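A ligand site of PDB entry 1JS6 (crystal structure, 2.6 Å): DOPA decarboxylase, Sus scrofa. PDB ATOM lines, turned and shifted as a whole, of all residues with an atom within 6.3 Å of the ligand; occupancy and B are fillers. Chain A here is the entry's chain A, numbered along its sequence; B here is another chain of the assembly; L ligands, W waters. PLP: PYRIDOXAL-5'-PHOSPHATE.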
ATOM      1  N   PHE A  80     -16.479  20.150  -6.121  1.00  0.00           N
ATOM      2  CA  PHE A  80     -15.042  20.411  -6.147  1.00  0.00           C
ATOM      3  C   PHE A  80     -14.462  19.322  -7.026  1.00  0.00           C
ATOM      4  O   PHE A  80     -15.113  18.331  -7.312  1.00  0.00           O
ATOM      5  CB  PHE A  80     -14.431  20.342  -4.743  1.00  0.00           C
ATOM      6  CG  PHE A  80     -14.482  21.654  -3.986  1.00  0.00           C
ATOM      7  CD1 PHE A  80     -14.777  21.679  -2.617  1.00  0.00           C
ATOM      8  CD2 PHE A  80     -14.200  22.866  -4.631  1.00  0.00           C
ATOM      9  CE1 PHE A  80     -14.816  22.885  -1.891  1.00  0.00           C
ATOM     10  CE2 PHE A  80     -14.227  24.087  -3.927  1.00  0.00           C
ATOM     11  CZ  PHE A  80     -14.535  24.097  -2.557  1.00  0.00           C
ATOM     12  N   GLY A 146      -9.579   7.302   4.888  1.00  0.00           N
ATOM     13  CA  GLY A 146     -10.429   7.026   3.742  1.00  0.00           C
ATOM     14  C   GLY A 146     -11.022   8.284   3.128  1.00  0.00           C
ATOM     15  O   GLY A 146     -11.254   8.369   1.924  1.00  0.00           O
ATOM     16  N   SER A 147     -11.272   9.283   3.960  1.00  0.00           N
ATOM     17  CA  SER A 147     -11.853  10.526   3.476  1.00  0.00           C
ATOM     18  C   SER A 147     -11.752  11.631   4.530  1.00  0.00           C
ATOM     19  O   SER A 147     -11.411  11.369   5.684  1.00  0.00           O
ATOM     20  CB  SER A 147     -13.312  10.296   3.102  1.00  0.00           C
ATOM     21  OG  SER A 147     -14.036   9.912   4.263  1.00  0.00           O
ATOM     22  N   ALA A 148     -12.041  12.864   4.122  1.00  0.00           N
ATOM     23  CA  ALA A 148     -11.969  13.962   5.068  1.00  0.00           C
ATOM     24  C   ALA A 148     -13.044  13.796   6.138  1.00  0.00           C
ATOM     25  O   ALA A 148     -12.817  14.150   7.297  1.00  0.00           O
ATOM     26  CB  ALA A 148     -12.146  15.264   4.360  1.00  0.00           C
ATOM     27  N   SER A 149     -14.193  13.233   5.777  1.00  0.00           N
ATOM     28  CA  SER A 149     -15.274  13.040   6.747  1.00  0.00           C
ATOM     29  C   SER A 149     -14.840  12.041   7.817  1.00  0.00           C
ATOM     30  O   SER A 149     -15.257  12.146   8.977  1.00  0.00           O
ATOM     31  CB  SER A 149     -16.551  12.529   6.086  1.00  0.00           C
ATOM     32  OG  SER A 149     -16.988  13.399   5.055  1.00  0.00           O
ATOM     33  N   GLU A 150     -14.020  11.068   7.441  1.00  0.00           N
ATOM     34  CA  GLU A 150     -13.560  10.093   8.409  1.00  0.00           C
ATOM     35  C   GLU A 150     -12.457  10.753   9.247  1.00  0.00           C
ATOM     36  O   GLU A 150     -12.403  10.598  10.475  1.00  0.00           O
ATOM     37  CB  GLU A 150     -13.071   8.854   7.687  1.00  0.00           C
ATOM     38  CG  GLU A 150     -14.143   8.268   6.777  1.00  0.00           C
ATOM     39  CD  GLU A 150     -13.670   7.064   5.976  1.00  0.00           C
ATOM     40  OE1 GLU A 150     -13.389   5.998   6.586  1.00  0.00           O
ATOM     41  OE2 GLU A 150     -13.565   7.173   4.734  1.00  0.00           O
ATOM     42  N   THR A 152     -12.152  13.817  10.099  1.00  0.00           N
ATOM     43  CA  THR A 152     -12.807  14.674  11.083  1.00  0.00           C
ATOM     44  C   THR A 152     -13.374  13.860  12.247  1.00  0.00           C
ATOM     45  O   THR A 152     -13.192  14.240  13.399  1.00  0.00           O
ATOM     46  CB  THR A 152     -13.934  15.491  10.439  1.00  0.00           C
ATOM     47  OG1 THR A 152     -13.385  16.385   9.468  1.00  0.00           O
ATOM     48  CG2 THR A 152     -14.686  16.290  11.481  1.00  0.00           C
ATOM     49  N   HIS A 192     -18.488  21.995   6.542  1.00  0.00           N
ATOM     50  CA  HIS A 192     -19.018  20.856   5.793  1.00  0.00           C
ATOM     51  C   HIS A 192     -19.924  19.988   6.674  1.00  0.00           C
ATOM     52  O   HIS A 192     -19.770  19.946   7.905  1.00  0.00           O
ATOM     53  CB  HIS A 192     -17.850  20.021   5.279  1.00  0.00           C
ATOM     54  CG  HIS A 192     -18.260  18.864   4.411  1.00  0.00           C
ATOM     55  ND1 HIS A 192     -18.472  18.988   3.054  1.00  0.00           N
ATOM     56  CD2 HIS A 192     -18.464  17.563   4.718  1.00  0.00           C
ATOM     57  CE1 HIS A 192     -18.778  17.804   2.559  1.00  0.00           C
ATOM     58  NE2 HIS A 192     -18.779  16.926   3.545  1.00  0.00           N
ATOM     59  N   SER A 194     -19.862  16.902   7.156  1.00  0.00           N
ATOM     60  CA  SER A 194     -19.116  15.832   7.798  1.00  0.00           C
ATOM     61  C   SER A 194     -18.933  16.100   9.301  1.00  0.00           C
ATOM     62  O   SER A 194     -18.777  15.179  10.083  1.00  0.00           O
ATOM     63  CB  SER A 194     -17.750  15.651   7.133  1.00  0.00           C
ATOM     64  OG  SER A 194     -16.981  16.844   7.199  1.00  0.00           O
ATOM     65  N   THR A 242     -12.204  25.564   9.203  1.00  0.00           N
ATOM     66  CA  THR A 242     -12.214  25.193   7.806  1.00  0.00           C
ATOM     67  C   THR A 242     -11.443  26.151   6.918  1.00  0.00           C
ATOM     68  O   THR A 242     -11.569  27.367   7.018  1.00  0.00           O
ATOM     69  CB  THR A 242     -13.659  25.115   7.283  1.00  0.00           C
ATOM     70  OG1 THR A 242     -14.403  24.167   8.079  1.00  0.00           O
ATOM     71  CG2 THR A 242     -13.681  24.658   5.846  1.00  0.00           C
ATOM     72  N   LEU A 243     -10.658  25.557   6.016  1.00  0.00           N
ATOM     73  CA  LEU A 243      -9.848  26.292   5.062  1.00  0.00           C
ATOM     74  C   LEU A 243     -10.311  25.890   3.662  1.00  0.00           C
ATOM     75  O   LEU A 243      -9.873  24.878   3.116  1.00  0.00           O
ATOM     76  CB  LEU A 243      -8.385  25.936   5.250  1.00  0.00           C
ATOM     77  CG  LEU A 243      -7.510  26.849   6.118  1.00  0.00           C
ATOM     78  CD1 LEU A 243      -8.257  27.284   7.357  1.00  0.00           C
ATOM     79  CD2 LEU A 243      -6.239  26.101   6.499  1.00  0.00           C
ATOM     80  N   GLY A 244     -11.203  26.694   3.089  1.00  0.00           N
ATOM     81  CA  GLY A 244     -11.728  26.428   1.756  1.00  0.00           C
ATOM     82  C   GLY A 244     -13.123  25.856   1.866  1.00  0.00           C
ATOM     83  O   GLY A 244     -13.377  24.761   1.387  1.00  0.00           O
ATOM     84  N   THR A 245     -14.029  26.579   2.528  1.00  0.00           N
ATOM     85  CA  THR A 245     -15.398  26.093   2.687  1.00  0.00           C
ATOM     86  C   THR A 245     -15.991  25.674   1.338  1.00  0.00           C
ATOM     87  O   THR A 245     -15.607  26.190   0.297  1.00  0.00           O
ATOM     88  CB  THR A 245     -16.292  27.164   3.352  1.00  0.00           C
ATOM     89  OG1 THR A 245     -16.267  28.367   2.597  1.00  0.00           O
ATOM     90  CG2 THR A 245     -15.803  27.477   4.729  1.00  0.00           C
ATOM     91  N   THR A 246     -16.909  24.711   1.376  1.00  0.00           N
ATOM     92  CA  THR A 246     -17.522  24.210   0.158  1.00  0.00           C
ATOM     93  C   THR A 246     -18.458  25.219  -0.519  1.00  0.00           C
ATOM     94  O   THR A 246     -18.648  25.187  -1.738  1.00  0.00           O
ATOM     95  CB  THR A 246     -18.276  22.893   0.420  1.00  0.00           C
ATOM     96  OG1 THR A 246     -19.284  23.102   1.398  1.00  0.00           O
ATOM     97  CG2 THR A 246     -17.329  21.838   0.926  1.00  0.00           C
ATOM     98  N   ASP A 271      -9.814  21.351   8.923  1.00  0.00           N
ATOM     99  CA  ASP A 271     -10.333  20.665   7.736  1.00  0.00           C
ATOM    100  C   ASP A 271     -10.103  21.555   6.520  1.00  0.00           C
ATOM    101  O   ASP A 271     -10.800  22.559   6.335  1.00  0.00           O
ATOM    102  CB  ASP A 271     -11.834  20.348   7.897  1.00  0.00           C
ATOM    103  CG  ASP A 271     -12.528  19.978   6.577  1.00  0.00           C
ATOM    104  OD1 ASP A 271     -11.841  19.741   5.555  1.00  0.00           O
ATOM    105  OD2 ASP A 271     -13.769  19.915   6.558  1.00  0.00           O
ATOM    106  N   ALA A 272      -9.106  21.195   5.713  1.00  0.00           N
ATOM    107  CA  ALA A 272      -8.781  21.936   4.488  1.00  0.00           C
ATOM    108  C   ALA A 272      -8.889  20.973   3.305  1.00  0.00           C
ATOM    109  O   ALA A 272      -8.086  21.013   2.376  1.00  0.00           O
ATOM    110  CB  ALA A 272      -7.376  22.485   4.567  1.00  0.00           C
ATOM    111  N   ALA A 273      -9.907  20.109   3.342  1.00  0.00           N
ATOM    112  CA  ALA A 273     -10.091  19.090   2.315  1.00  0.00           C
ATOM    113  C   ALA A 273      -9.742  19.452   0.885  1.00  0.00           C
ATOM    114  O   ALA A 273      -9.014  18.711   0.197  1.00  0.00           O
ATOM    115  CB  ALA A 273     -11.506  18.546   2.367  1.00  0.00           C
ATOM    116  N   TYR A 274     -10.270  20.585   0.435  1.00  0.00           N
ATOM    117  CA  TYR A 274     -10.050  21.051  -0.914  1.00  0.00           C
ATOM    118  C   TYR A 274      -8.846  21.971  -1.066  1.00  0.00           C
ATOM    119  O   TYR A 274      -7.904  21.663  -1.808  1.00  0.00           O
ATOM    120  CB  TYR A 274     -11.301  21.773  -1.427  1.00  0.00           C
ATOM    121  CG  TYR A 274     -11.068  22.522  -2.715  1.00  0.00           C
ATOM    122  CD1 TYR A 274     -10.726  21.846  -3.892  1.00  0.00           C
ATOM    123  CD2 TYR A 274     -11.104  23.917  -2.751  1.00  0.00           C
ATOM    124  CE1 TYR A 274     -10.444  22.547  -5.064  1.00  0.00           C
ATOM    125  CE2 TYR A 274     -10.835  24.617  -3.911  1.00  0.00           C
ATOM    126  CZ  TYR A 274     -10.498  23.933  -5.068  1.00  0.00           C
ATOM    127  OH  TYR A 274     -10.221  24.627  -6.229  1.00  0.00           O
ATOM    128  N   ALA A 275      -8.882  23.108  -0.361  1.00  0.00           N
ATOM    129  CA  ALA A 275      -7.822  24.103  -0.461  1.00  0.00           C
ATOM    130  C   ALA A 275      -6.422  23.641  -0.088  1.00  0.00           C
ATOM    131  O   ALA A 275      -5.432  24.197  -0.556  1.00  0.00           O
ATOM    132  CB  ALA A 275      -8.182  25.315   0.341  1.00  0.00           C
ATOM    133  N   ASN A 300      -7.551  16.626   1.354  1.00  0.00           N
ATOM    134  CA  ASN A 300      -7.705  15.508   0.435  1.00  0.00           C
ATOM    135  C   ASN A 300      -6.871  15.512  -0.848  1.00  0.00           C
ATOM    136  O   ASN A 300      -7.095  16.310  -1.767  1.00  0.00           O
ATOM    137  CB  ASN A 300      -9.165  15.357   0.022  1.00  0.00           C
ATOM    138  CG  ASN A 300     -10.044  14.892   1.134  1.00  0.00           C
ATOM    139  OD1 ASN A 300      -9.651  14.085   1.958  1.00  0.00           O
ATOM    140  ND2 ASN A 300     -11.272  15.389   1.159  1.00  0.00           N
ATOM    141  N   HIS A 302      -7.069  13.342  -2.846  1.00  0.00           N
ATOM    142  CA  HIS A 302      -7.990  12.768  -3.818  1.00  0.00           C
ATOM    143  C   HIS A 302      -9.006  13.776  -4.339  1.00  0.00           C
ATOM    144  O   HIS A 302      -9.963  13.422  -5.035  1.00  0.00           O
ATOM    145  CB  HIS A 302      -8.682  11.466  -3.300  1.00  0.00           C
ATOM    146  CG  HIS A 302      -9.679  11.659  -2.193  1.00  0.00           C
ATOM    147  ND1 HIS A 302      -9.823  10.735  -1.175  1.00  0.00           N
ATOM    148  CD2 HIS A 302     -10.601  12.620  -1.959  1.00  0.00           C
ATOM    149  CE1 HIS A 302     -10.786  11.119  -0.360  1.00  0.00           C
ATOM    150  NE2 HIS A 302     -11.279  12.261  -0.812  1.00  0.00           N
ATOM    151  N   LYS A 303      -8.789  15.040  -4.005  1.00  0.00           N
ATOM    152  CA  LYS A 303      -9.639  16.088  -4.539  1.00  0.00           C
ATOM    153  C   LYS A 303      -8.815  16.888  -5.534  1.00  0.00           C
ATOM    154  O   LYS A 303      -8.966  16.717  -6.737  1.00  0.00           O
ATOM    155  CB  LYS A 303     -10.169  17.015  -3.455  1.00  0.00           C
ATOM    156  CG  LYS A 303     -11.551  16.652  -3.013  1.00  0.00           C
ATOM    157  CD  LYS A 303     -12.227  17.765  -2.246  1.00  0.00           C
ATOM    158  CE  LYS A 303     -13.571  17.291  -1.768  1.00  0.00           C
ATOM    159  NZ  LYS A 303     -14.127  18.246  -0.801  1.00  0.00           N
ATOM    160  N   PHE A 309      -9.329   8.827  -5.887  1.00  0.00           N
ATOM    161  CA  PHE A 309     -10.089   8.609  -4.672  1.00  0.00           C
ATOM    162  C   PHE A 309      -9.819   7.377  -3.891  1.00  0.00           C
ATOM    163  O   PHE A 309      -9.741   6.255  -4.418  1.00  0.00           O
ATOM    164  CB  PHE A 309     -11.595   8.658  -4.869  1.00  0.00           C
ATOM    165  CG  PHE A 309     -12.371   8.445  -3.582  1.00  0.00           C
ATOM    166  CD1 PHE A 309     -12.860   7.195  -3.231  1.00  0.00           C
ATOM    167  CD2 PHE A 309     -12.586   9.510  -2.693  1.00  0.00           C
ATOM    168  CE1 PHE A 309     -13.558   7.003  -2.021  1.00  0.00           C
ATOM    169  CE2 PHE A 309     -13.279   9.326  -1.504  1.00  0.00           C
ATOM    170  CZ  PHE A 309     -13.760   8.055  -1.163  1.00  0.00           C
ATOM    171  N   SER A 312      -7.113  10.505   1.771  1.00  0.00           N
ATOM    172  CA  SER A 312      -7.191  11.736   2.550  1.00  0.00           C
ATOM    173  C   SER A 312      -5.957  11.730   3.461  1.00  0.00           C
ATOM    174  O   SER A 312      -5.651  10.694   4.070  1.00  0.00           O
ATOM    175  CB  SER A 312      -8.475  11.750   3.388  1.00  0.00           C
ATOM    176  OG  SER A 312      -8.566  12.939   4.157  1.00  0.00           O
ATOM    177  N   ILE B 101     -17.566   9.840  -7.739  1.00  0.00           N
ATOM    178  CA  ILE B 101     -17.696   9.741  -6.284  1.00  0.00           C
ATOM    179  C   ILE B 101     -19.182   9.657  -6.002  1.00  0.00           C
ATOM    180  O   ILE B 101     -19.868  10.673  -6.048  1.00  0.00           O
ATOM    181  CB  ILE B 101     -17.126  10.975  -5.569  1.00  0.00           C
ATOM    182  CG1 ILE B 101     -15.636  11.095  -5.861  1.00  0.00           C
ATOM    183  CG2 ILE B 101     -17.322  10.870  -4.059  1.00  0.00           C
ATOM    184  CD1 ILE B 101     -14.822   9.932  -5.325  1.00  0.00           C
ATOM    185  N   PRO B 352     -18.590   7.157   6.151  1.00  0.00           N
ATOM    186  CA  PRO B 352     -18.112   8.223   5.257  1.00  0.00           C
ATOM    187  C   PRO B 352     -19.172   8.737   4.295  1.00  0.00           C
ATOM    188  O   PRO B 352     -20.177   8.084   4.061  1.00  0.00           O
ATOM    189  CB  PRO B 352     -16.951   7.554   4.524  1.00  0.00           C
ATOM    190  CG  PRO B 352     -17.443   6.154   4.373  1.00  0.00           C
ATOM    191  CD  PRO B 352     -17.999   5.863   5.751  1.00  0.00           C
ATOM    192  N   LEU B 353     -18.917   9.911   3.711  1.00  0.00           N
ATOM    193  CA  LEU B 353     -19.847  10.484   2.749  1.00  0.00           C
ATOM    194  C   LEU B 353     -19.502  10.003   1.332  1.00  0.00           C
ATOM    195  O   LEU B 353     -20.389   9.612   0.589  1.00  0.00           O
ATOM    196  CB  LEU B 353     -19.807  12.032   2.808  1.00  0.00           C
ATOM    197  CG  LEU B 353     -20.865  12.777   3.633  1.00  0.00           C
ATOM    198  CD1 LEU B 353     -21.815  11.775   4.296  1.00  0.00           C
ATOM    199  CD2 LEU B 353     -20.192  13.638   4.689  1.00  0.00           C
ATOM    200  N   GLY B 354     -18.225  10.024   0.966  1.00  0.00           N
ATOM    201  CA  GLY B 354     -17.856   9.593  -0.362  1.00  0.00           C
ATOM    202  C   GLY B 354     -17.755   8.078  -0.513  1.00  0.00           C
ATOM    203  O   GLY B 354     -17.824   7.365   0.480  1.00  0.00           O
HETATM  204  N1  PLP L   1     -14.797  18.992   4.076  1.00  0.00           N
HETATM  205  C2  PLP L   1     -14.586  19.927   3.103  1.00  0.00           C
HETATM  206  C2A PLP L   1     -14.123  21.314   3.508  1.00  0.00           C
HETATM  207  C3  PLP L   1     -14.721  19.588   1.777  1.00  0.00           C
HETATM  208  O3  PLP L   1     -14.482  20.525   0.802  1.00  0.00           O
HETATM  209  C4  PLP L   1     -15.065  18.301   1.424  1.00  0.00           C
HETATM  210  C4A PLP L   1     -15.093  17.901  -0.042  1.00  0.00           C
HETATM  211  C5  PLP L   1     -15.267  17.359   2.416  1.00  0.00           C
HETATM  212  C6  PLP L   1     -15.127  17.705   3.732  1.00  0.00           C
HETATM  213  C5A PLP L   1     -15.615  15.901   2.052  1.00  0.00           C
HETATM  214  O4P PLP L   1     -14.429  15.135   1.818  1.00  0.00           O
HETATM  215  P   PLP L   1     -14.525  13.558   1.562  1.00  0.00           P
HETATM  216  O1P PLP L   1     -13.154  13.015   1.515  1.00  0.00           O
HETATM  217  O2P PLP L   1     -15.232  13.038   2.911  1.00  0.00           O
HETATM  218  O3P PLP L   1     -15.441  13.327   0.422  1.00  0.00           O
HETATM  219  O   HOH W   1     -16.532  10.737   2.969  1.00  0.00           O
HETATM  220  O   HOH W   2     -17.615  14.470  -0.223  1.00  0.00           O
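The side-chain carboxylate (OD2) of Asp 271 is in hydrogen-bond range of a nitrogen (N1) of the ligand, at 2.8 Å.
An oxygen (O1P) of the ligand lies within hydrogen-bond range of the backbone NH (N) of Ala 148 (2.8 Å).
O2P of the ligand is in hydrogen-bond range of OG of Ser 149 (2.8 Å).
O1P of the ligand is in hydrogen-bond range of NE2 of His 302, 3.1 Å away.
The backbone NH (N) of Ser 149 lies within hydrogen-bond range of an oxygen (O2P) of the ligand.
An oxygen (O1P) of the ligand sits at hydrogen-bond distance from the side-chain amide nitrogen of Asn 300, at 3.1 Å.
C4A of the ligand is bonded to NZ of Lys 303 (1.3 Å).
OG of Ser 312 is in hydrogen-bond range of N of Ala 148, at 3.5 Å.
O of Ala 148 lies within hydrogen-bond range of OG1 of Thr 152 (3.2 Å).
The backbone NH (N) of Leu 243 sits at hydrogen-bond distance from the backbone carbonyl oxygen (O) of Asp 271 (3.0 Å).
OD1 of Asn 300 sits at hydrogen-bond distance from N of Ala 148 (3.4 Å).
OE2 of Glu 150 is in hydrogen-bond range of OG of Ser 147 (2.8 Å).
The backbone NH (N) of Asn 300 lies within hydrogen-bond range of the backbone carbonyl oxygen (O) of Ala 273 (2.8 Å).
The side-chain hydroxyl of Ser 312 lies within hydrogen-bond range of the side-chain amide oxygen of Asn 300.
OD1 of Asp 271 is in hydrogen-bond range of N of Ala 273 (3.0 Å).
Phe 80 touches the ligand.
Ser 147 touches the ligand (CB to O1P, 3.2 Å).
His 192 touches the ligand (CG to C6, 3.4 Å).
Thr 246 touches the ligand (CG2 to O3, 3.1 Å).
CB of Ala 273 touches C3 of the ligand, at 3.4 Å.
Hydrophobic or aromatic side chains within 4 Å of the ligand: Phe 80, Ala 148, His 192, Ala 273 and His 302.
Within 4 Å of the ligand: Phe 80, Ser 147, Ala 148, Ser 149, His 192, Thr 246, Asp 271, Ala 273, Asn 300, His 302 and Lys 303.
Along chain A the residues within 4 Å of the ligand span positions 80 to 303.
Water W1 lies within hydrogen-bond range of N of Leu 353 of chain B (2.6 Å), O2P of the ligand (2.6 Å), N of Gly 354 of chain B (2.7 Å), OG of Ser 147 (2.9 Å) and OG of Ser 149 (3.4 Å).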
